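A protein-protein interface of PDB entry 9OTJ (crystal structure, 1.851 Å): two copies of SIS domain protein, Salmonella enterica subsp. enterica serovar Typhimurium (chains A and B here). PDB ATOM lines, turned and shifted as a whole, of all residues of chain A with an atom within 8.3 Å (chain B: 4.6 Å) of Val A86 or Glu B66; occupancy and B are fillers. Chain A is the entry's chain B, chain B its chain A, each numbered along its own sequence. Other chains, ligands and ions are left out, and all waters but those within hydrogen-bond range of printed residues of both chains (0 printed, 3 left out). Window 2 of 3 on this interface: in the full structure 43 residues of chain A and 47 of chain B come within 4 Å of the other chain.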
ATOM      1  N   HIS A  43     -32.407 -24.847   1.647  1.00  0.00           N
ATOM      2  CA  HIS A  43     -32.270 -24.679   3.070  1.00  0.00           C
ATOM      3  C   HIS A  43     -33.651 -24.398   3.652  1.00  0.00           C
ATOM      4  O   HIS A  43     -34.409 -23.575   3.119  1.00  0.00           O
ATOM      5  CB  HIS A  43     -31.242 -23.616   3.454  1.00  0.00           C
ATOM      6  CG  HIS A  43     -29.921 -23.796   2.793  1.00  0.00           C
ATOM      7  ND1 HIS A  43     -29.619 -22.988   1.703  1.00  0.00           N
ATOM      8  CD2 HIS A  43     -28.865 -24.572   2.995  1.00  0.00           C
ATOM      9  CE1 HIS A  43     -28.419 -23.318   1.245  1.00  0.00           C
ATOM     10  NE2 HIS A  43     -27.932 -24.293   1.974  1.00  0.00           N
ATOM     11  N   TYR A  45     -35.346 -23.324   7.410  1.00  0.00           N
ATOM     12  CA  TYR A  45     -35.136 -22.857   8.768  1.00  0.00           C
ATOM     13  C   TYR A  45     -36.479 -22.736   9.474  1.00  0.00           C
ATOM     14  O   TYR A  45     -37.418 -22.101   8.963  1.00  0.00           O
ATOM     15  CB  TYR A  45     -34.428 -21.497   8.829  1.00  0.00           C
ATOM     16  CG  TYR A  45     -33.034 -21.592   8.236  1.00  0.00           C
ATOM     17  CD1 TYR A  45     -31.990 -22.222   8.912  1.00  0.00           C
ATOM     18  CD2 TYR A  45     -32.773 -21.041   6.989  1.00  0.00           C
ATOM     19  CE1 TYR A  45     -30.729 -22.322   8.338  1.00  0.00           C
ATOM     20  CE2 TYR A  45     -31.511 -21.103   6.430  1.00  0.00           C
ATOM     21  CZ  TYR A  45     -30.513 -21.796   7.069  1.00  0.00           C
ATOM     22  OH  TYR A  45     -29.354 -21.880   6.359  1.00  0.00           O
ATOM     23  N   TYR A  75     -34.101 -22.962  15.091  1.00  0.00           N
ATOM     24  CA  TYR A  75     -33.466 -21.865  15.800  1.00  0.00           C
ATOM     25  C   TYR A  75     -34.459 -21.231  16.759  1.00  0.00           C
ATOM     26  O   TYR A  75     -35.643 -21.134  16.495  1.00  0.00           O
ATOM     27  CB  TYR A  75     -33.039 -20.691  14.911  1.00  0.00           C
ATOM     28  CG  TYR A  75     -31.786 -20.903  14.089  1.00  0.00           C
ATOM     29  CD1 TYR A  75     -31.776 -21.751  12.977  1.00  0.00           C
ATOM     30  CD2 TYR A  75     -30.623 -20.214  14.390  1.00  0.00           C
ATOM     31  CE1 TYR A  75     -30.617 -21.933  12.231  1.00  0.00           C
ATOM     32  CE2 TYR A  75     -29.470 -20.338  13.630  1.00  0.00           C
ATOM     33  CZ  TYR A  75     -29.465 -21.217  12.554  1.00  0.00           C
ATOM     34  OH  TYR A  75     -28.294 -21.264  11.862  1.00  0.00           O
ATOM     35  N   ASN A  83     -27.651 -14.112  15.074  1.00  0.00           N
ATOM     36  CA  ASN A  83     -26.580 -14.826  14.412  1.00  0.00           C
ATOM     37  C   ASN A  83     -27.113 -15.640  13.226  1.00  0.00           C
ATOM     38  O   ASN A  83     -27.090 -16.873  13.198  1.00  0.00           O
ATOM     39  CB  ASN A  83     -25.847 -15.659  15.445  1.00  0.00           C
ATOM     40  CG  ASN A  83     -24.560 -16.197  14.890  1.00  0.00           C
ATOM     41  OD1 ASN A  83     -23.853 -15.507  14.158  1.00  0.00           O
ATOM     42  ND2 ASN A  83     -24.251 -17.427  15.212  1.00  0.00           N
ATOM     43  N   PRO A  84     -27.646 -14.979  12.192  1.00  0.00           N
ATOM     44  CA  PRO A  84     -28.258 -15.703  11.101  1.00  0.00           C
ATOM     45  C   PRO A  84     -27.249 -16.478  10.298  1.00  0.00           C
ATOM     46  O   PRO A  84     -26.138 -16.037  10.181  1.00  0.00           O
ATOM     47  CB  PRO A  84     -28.882 -14.616  10.260  1.00  0.00           C
ATOM     48  CG  PRO A  84     -28.093 -13.393  10.636  1.00  0.00           C
ATOM     49  CD  PRO A  84     -27.848 -13.532  12.083  1.00  0.00           C
ATOM     50  N   PRO A  85     -27.618 -17.647   9.749  1.00  0.00           N
ATOM     51  CA  PRO A  85     -26.657 -18.459   9.033  1.00  0.00           C
ATOM     52  C   PRO A  85     -26.305 -17.761   7.737  1.00  0.00           C
ATOM     53  O   PRO A  85     -27.196 -17.114   7.195  1.00  0.00           O
ATOM     54  CB  PRO A  85     -27.388 -19.783   8.899  1.00  0.00           C
ATOM     55  CG  PRO A  85     -28.845 -19.466   9.036  1.00  0.00           C
ATOM     56  CD  PRO A  85     -28.954 -18.231   9.819  1.00  0.00           C
ATOM     57  N   VAL A  86     -25.090 -17.972   7.212  1.00  0.00           N
ATOM     58  CA  VAL A  86     -24.739 -17.377   5.932  1.00  0.00           C
ATOM     59  C   VAL A  86     -25.594 -17.980   4.836  1.00  0.00           C
ATOM     60  O   VAL A  86     -25.814 -17.311   3.853  1.00  0.00           O
ATOM     61  CB  VAL A  86     -23.238 -17.481   5.619  1.00  0.00           C
ATOM     62  CG1 VAL A  86     -22.450 -16.883   6.768  1.00  0.00           C
ATOM     63  CG2 VAL A  86     -22.772 -18.895   5.377  1.00  0.00           C
ATOM     64  N   ALA A  87     -26.155 -19.191   5.006  1.00  0.00           N
ATOM     65  CA  ALA A  87     -27.019 -19.738   3.958  1.00  0.00           C
ATOM     66  C   ALA A  87     -28.393 -19.069   3.906  1.00  0.00           C
ATOM     67  O   ALA A  87     -29.200 -19.414   3.056  1.00  0.00           O
ATOM     68  CB  ALA A  87     -27.151 -21.241   4.092  1.00  0.00           C
ATOM     69  N   LEU A  88     -28.705 -18.144   4.820  1.00  0.00           N
ATOM     70  CA  LEU A  88     -29.986 -17.450   4.756  1.00  0.00           C
ATOM     71  C   LEU A  88     -29.963 -16.605   3.505  1.00  0.00           C
ATOM     72  O   LEU A  88     -29.088 -15.767   3.385  1.00  0.00           O
ATOM     73  CB  LEU A  88     -30.196 -16.525   5.933  1.00  0.00           C
ATOM     74  CG  LEU A  88     -31.543 -15.826   5.966  1.00  0.00           C
ATOM     75  CD1 LEU A  88     -32.672 -16.884   5.890  1.00  0.00           C
ATOM     76  CD2 LEU A  88     -31.594 -14.967   7.234  1.00  0.00           C
ATOM     77  N   GLY A  89     -30.926 -16.822   2.616  1.00  0.00           N
ATOM     78  CA  GLY A  89     -30.828 -16.290   1.278  1.00  0.00           C
ATOM     79  C   GLY A  89     -31.964 -16.745   0.384  1.00  0.00           C
ATOM     80  O   GLY A  89     -32.942 -17.340   0.848  1.00  0.00           O
ATOM     81  N   GLU A  90     -31.813 -16.424  -0.904  1.00  0.00           N
ATOM     82  CA  GLU A  90     -32.823 -16.742  -1.898  1.00  0.00           C
ATOM     83  C   GLU A  90     -33.079 -18.243  -2.054  1.00  0.00           C
ATOM     84  O   GLU A  90     -34.110 -18.614  -2.626  1.00  0.00           O
ATOM     85  CB  GLU A  90     -32.536 -16.080  -3.252  1.00  0.00           C
ATOM     86  CG  GLU A  90     -31.288 -16.553  -3.986  1.00  0.00           C
ATOM     87  CD  GLU A  90     -30.939 -15.695  -5.210  1.00  0.00           C
ATOM     88  OE1 GLU A  90     -30.008 -16.106  -5.946  1.00  0.00           O
ATOM     89  OE2 GLU A  90     -31.610 -14.650  -5.454  1.00  0.00           O
ATOM     90  N   ALA A  92     -33.225 -20.300   0.632  1.00  0.00           N
ATOM     91  CA  ALA A  92     -33.671 -20.711   1.940  1.00  0.00           C
ATOM     92  C   ALA A  92     -35.160 -20.357   2.033  1.00  0.00           C
ATOM     93  O   ALA A  92     -35.586 -19.325   1.507  1.00  0.00           O
ATOM     94  CB  ALA A  92     -32.892 -20.009   3.052  1.00  0.00           C
ATOM     95  N   HIS A 116     -33.119 -10.801   3.249  1.00  0.00           N
ATOM     96  CA  HIS A 116     -32.135 -11.603   2.537  1.00  0.00           C
ATOM     97  C   HIS A 116     -32.761 -12.293   1.340  1.00  0.00           C
ATOM     98  O   HIS A 116     -32.121 -13.077   0.654  1.00  0.00           O
ATOM     99  CB  HIS A 116     -31.525 -12.668   3.447  1.00  0.00           C
ATOM    100  CG  HIS A 116     -30.657 -12.130   4.512  1.00  0.00           C
ATOM    101  ND1 HIS A 116     -31.094 -11.341   5.547  1.00  0.00           N
ATOM    102  CD2 HIS A 116     -29.372 -12.380   4.753  1.00  0.00           C
ATOM    103  CE1 HIS A 116     -30.069 -11.092   6.350  1.00  0.00           C
ATOM    104  NE2 HIS A 116     -29.027 -11.715   5.890  1.00  0.00           N
ATOM    105  N   PHE B  62     -20.821 -24.281  14.262  1.00  0.00           N
ATOM    106  CA  PHE B  62     -19.966 -23.820  13.158  1.00  0.00           C
ATOM    107  C   PHE B  62     -20.543 -24.082  11.751  1.00  0.00           C
ATOM    108  O   PHE B  62     -20.636 -23.170  10.931  1.00  0.00           O
ATOM    109  CB  PHE B  62     -18.585 -24.489  13.302  1.00  0.00           C
ATOM    110  CG  PHE B  62     -17.590 -24.021  12.257  1.00  0.00           C
ATOM    111  CD1 PHE B  62     -16.796 -22.899  12.443  1.00  0.00           C
ATOM    112  CD2 PHE B  62     -17.465 -24.696  11.052  1.00  0.00           C
ATOM    113  CE1 PHE B  62     -15.924 -22.452  11.450  1.00  0.00           C
ATOM    114  CE2 PHE B  62     -16.612 -24.229  10.063  1.00  0.00           C
ATOM    115  CZ  PHE B  62     -15.820 -23.128  10.262  1.00  0.00           C
ATOM    116  N   LEU B  63     -20.831 -25.345  11.419  1.00  0.00           N
ATOM    117  CA  LEU B  63     -21.352 -25.690  10.125  1.00  0.00           C
ATOM    118  C   LEU B  63     -22.743 -25.084   9.889  1.00  0.00           C
ATOM    119  O   LEU B  63     -23.024 -24.685   8.775  1.00  0.00           O
ATOM    120  CB  LEU B  63     -21.299 -27.198   9.898  1.00  0.00           C
ATOM    121  CG  LEU B  63     -19.894 -27.766   9.715  1.00  0.00           C
ATOM    122  CD1 LEU B  63     -19.937 -29.274   9.554  1.00  0.00           C
ATOM    123  CD2 LEU B  63     -19.159 -27.107   8.560  1.00  0.00           C
ATOM    124  N   GLU B  64     -23.600 -24.951  10.892  1.00  0.00           N
ATOM    125  CA  GLU B  64     -24.879 -24.317  10.666  1.00  0.00           C
ATOM    126  C   GLU B  64     -24.684 -22.846  10.315  1.00  0.00           C
ATOM    127  O   GLU B  64     -25.397 -22.348   9.441  1.00  0.00           O
ATOM    128  CB  GLU B  64     -25.884 -24.485  11.790  1.00  0.00           C
ATOM    129  CG  GLU B  64     -26.289 -25.940  12.016  1.00  0.00           C
ATOM    130  CD  GLU B  64     -27.473 -26.094  12.972  1.00  0.00           C
ATOM    131  OE1 GLU B  64     -27.535 -25.366  13.998  1.00  0.00           O
ATOM    132  OE2 GLU B  64     -28.322 -26.969  12.686  1.00  0.00           O
ATOM    133  N   LYS B  65     -23.735 -22.184  11.013  1.00  0.00           N
ATOM    134  CA  LYS B  65     -23.480 -20.776  10.752  1.00  0.00           C
ATOM    135  C   LYS B  65     -22.784 -20.580   9.408  1.00  0.00           C
ATOM    136  O   LYS B  65     -23.140 -19.712   8.654  1.00  0.00           O
ATOM    137  CB  LYS B  65     -22.674 -20.148  11.895  1.00  0.00           C
ATOM    138  CG  LYS B  65     -22.119 -18.763  11.617  1.00  0.00           C
ATOM    139  CD  LYS B  65     -23.306 -17.824  11.416  1.00  0.00           C
ATOM    140  CE  LYS B  65     -22.973 -16.566  10.709  1.00  0.00           C
ATOM    141  NZ  LYS B  65     -22.334 -15.703  11.685  1.00  0.00           N
ATOM    142  N   GLU B  66     -21.780 -21.381   9.101  1.00  0.00           N
ATOM    143  CA  GLU B  66     -20.792 -20.991   8.112  1.00  0.00           C
ATOM    144  C   GLU B  66     -20.981 -21.676   6.753  1.00  0.00           C
ATOM    145  O   GLU B  66     -20.411 -21.190   5.804  1.00  0.00           O
ATOM    146  CB  GLU B  66     -19.378 -21.343   8.609  1.00  0.00           C
ATOM    147  CG  GLU B  66     -18.955 -20.701   9.920  1.00  0.00           C
ATOM    148  CD  GLU B  66     -18.791 -19.172   9.922  1.00  0.00           C
ATOM    149  OE1 GLU B  66     -18.756 -18.620  11.032  1.00  0.00           O
ATOM    150  OE2 GLU B  66     -18.716 -18.563   8.844  1.00  0.00           O
ATOM    151  N   ALA B  67     -21.631 -22.864   6.662  1.00  0.00           N
ATOM    152  CA  ALA B  67     -21.687 -23.651   5.436  1.00  0.00           C
ATOM    153  C   ALA B  67     -22.854 -23.234   4.561  1.00  0.00           C
ATOM    154  O   ALA B  67     -23.903 -22.885   5.081  1.00  0.00           O
ATOM    155  CB  ALA B  67     -21.814 -25.148   5.755  1.00  0.00           C
ATOM    156  N   LYS B  68     -22.674 -23.359   3.233  1.00  0.00           N
ATOM    157  CA  LYS B  68     -23.752 -23.248   2.257  1.00  0.00           C
ATOM    158  C   LYS B  68     -24.076 -24.554   1.538  1.00  0.00           C
ATOM    159  O   LYS B  68     -25.134 -24.665   0.969  1.00  0.00           O
ATOM    160  CB  LYS B  68     -23.391 -22.197   1.199  1.00  0.00           C
ATOM    161  CG  LYS B  68     -23.250 -20.807   1.803  1.00  0.00           C
ATOM    162  CD  LYS B  68     -23.330 -19.626   0.836  1.00  0.00           C
ATOM    163  CE  LYS B  68     -22.046 -19.338   0.135  1.00  0.00           C
ATOM    164  NZ  LYS B  68     -21.001 -18.958   1.091  1.00  0.00           N
ATOM    165  N   LEU B 165     -15.033 -27.796   5.825  1.00  0.00           N
ATOM    166  CA  LEU B 165     -15.590 -26.649   5.125  1.00  0.00           C
ATOM    167  C   LEU B 165     -14.497 -26.046   4.239  1.00  0.00           C
ATOM    168  O   LEU B 165     -14.722 -25.789   3.064  1.00  0.00           O
ATOM    169  CB  LEU B 165     -16.171 -25.600   6.073  1.00  0.00           C
ATOM    170  CG  LEU B 165     -16.833 -24.387   5.404  1.00  0.00           C
ATOM    171  CD1 LEU B 165     -18.183 -24.722   4.816  1.00  0.00           C
ATOM    172  CD2 LEU B 165     -16.932 -23.287   6.400  1.00  0.00           C
ATOM    173  N   TYR B 171     -13.515 -21.551   3.353  1.00  0.00           N
ATOM    174  CA  TYR B 171     -13.914 -20.872   4.559  1.00  0.00           C
ATOM    175  C   TYR B 171     -13.146 -19.567   4.641  1.00  0.00           C
ATOM    176  O   TYR B 171     -11.930 -19.589   4.828  1.00  0.00           O
ATOM    177  CB  TYR B 171     -13.545 -21.752   5.751  1.00  0.00           C
ATOM    178  CG  TYR B 171     -13.768 -21.079   7.105  1.00  0.00           C
ATOM    179  CD1 TYR B 171     -14.862 -20.257   7.313  1.00  0.00           C
ATOM    180  CD2 TYR B 171     -12.915 -21.328   8.169  1.00  0.00           C
ATOM    181  CE1 TYR B 171     -15.131 -19.718   8.558  1.00  0.00           C
ATOM    182  CE2 TYR B 171     -13.148 -20.776   9.414  1.00  0.00           C
ATOM    183  CZ  TYR B 171     -14.233 -19.942   9.588  1.00  0.00           C
ATOM    184  OH  TYR B 171     -14.474 -19.404  10.799  1.00  0.00           O
ATOM    185  N   HIS B 173     -12.734 -17.422   6.864  1.00  0.00           N
ATOM    186  CA  HIS B 173     -12.058 -16.964   8.087  1.00  0.00           C
ATOM    187  C   HIS B 173     -11.074 -17.991   8.608  1.00  0.00           C
ATOM    188  O   HIS B 173     -10.767 -18.033   9.812  1.00  0.00           O
ATOM    189  CB  HIS B 173     -13.049 -16.497   9.162  1.00  0.00           C
ATOM    190  CG  HIS B 173     -14.018 -15.486   8.663  1.00  0.00           C
ATOM    191  ND1 HIS B 173     -13.607 -14.276   8.155  1.00  0.00           N
ATOM    192  CD2 HIS B 173     -15.336 -15.517   8.508  1.00  0.00           C
ATOM    193  CE1 HIS B 173     -14.662 -13.604   7.729  1.00  0.00           C
ATOM    194  NE2 HIS B 173     -15.729 -14.319   7.967  1.00  0.00           N
ATOM    195  N   THR B 305     -14.559 -12.592  13.973  1.00  0.00           N
ATOM    196  CA  THR B 305     -14.973 -13.503  12.915  1.00  0.00           C
ATOM    197  C   THR B 305     -15.147 -14.946  13.416  1.00  0.00           C
ATOM    198  O   THR B 305     -15.944 -15.702  12.841  1.00  0.00           O
ATOM    199  CB  THR B 305     -13.980 -13.400  11.761  1.00  0.00           C
ATOM    200  OG1 THR B 305     -12.703 -13.684  12.308  1.00  0.00           O
ATOM    201  CG2 THR B 305     -14.008 -12.055  11.045  1.00  0.00           C
ATOM    202  N   TYR B 309     -16.670 -19.538  18.443  1.00  0.00           N
ATOM    203  CA  TYR B 309     -16.335 -20.951  18.481  1.00  0.00           C
ATOM    204  C   TYR B 309     -15.342 -21.310  19.583  1.00  0.00           C
ATOM    205  O   TYR B 309     -15.085 -22.511  19.761  1.00  0.00           O
ATOM    206  CB  TYR B 309     -15.823 -21.334  17.093  1.00  0.00           C
ATOM    207  CG  TYR B 309     -16.814 -20.997  16.000  1.00  0.00           C
ATOM    208  CD1 TYR B 309     -18.123 -21.481  16.036  1.00  0.00           C
ATOM    209  CD2 TYR B 309     -16.467 -20.145  14.989  1.00  0.00           C
ATOM    210  CE1 TYR B 309     -19.059 -21.090  15.098  1.00  0.00           C
ATOM    211  CE2 TYR B 309     -17.396 -19.755  14.046  1.00  0.00           C
ATOM    212  CZ  TYR B 309     -18.699 -20.198  14.110  1.00  0.00           C
ATOM    213  OH  TYR B 309     -19.564 -19.776  13.141  1.00  0.00           O
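The side-chain amide oxygen (OD1) of Asn A83 sits at hydrogen-bond distance from the side-chain amino group (NZ) of Lys B65. The backbone carbonyl oxygen of Lys B65 is in hydrogen-bond range of the backbone NH of Val A86 (3.0 Å). The backbone carbonyl oxygen (O) of Lys B68 sits at hydrogen-bond distance from a ring nitrogen (NE2) of His A43 (3.0 Å).
OH of Tyr B309 sits at hydrogen-bond distance from OE1 of Glu B66 (2.5 Å).
Among the printed residues, pairs that only touch across the chains: Pro A84 with Lys B65 (3.3 Å), Pro A85 with Glu B64 (3.3 Å), Val A86 with Glu B66 (3.3 Å), Pro A85 with Lys B65 (3.8 Å), Ala A87 with Ala B67 (3.8 Å) and Tyr A75 with Glu B64 (3.9 Å).
Printed residues of chain B within 4 Å of His A43: Lys B68 (3.0 Å). Of the printed residues of chain B, Asn A83 touches Lys B65 (2.9 Å). Val A86 touches just these residues of chain B: Lys B65 (3.0 Å) and Glu B66 (3.3 Å). Of chain A, only Val A86 comes within 4 Å of Glu B66. Of chain A, only Ala A87 (3.8 Å) comes within 4 Å of Ala B67. The nearest residue of chain A that does not touch Glu B66 is Pro A85 (5.7 Å).
Hydrophobic or aromatic side chains of chain A that line the printed part of chain B: His A43, Tyr A75, Pro A85, Val A86 and Ala A87. Printed residues of chain B that touch a printed residue of chain A: Glu B64, Lys B65, Glu B66, Ala B67 and Lys B68. Among the printed residues, 9 pairs touch across the chains.
No position is printed for both chains.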
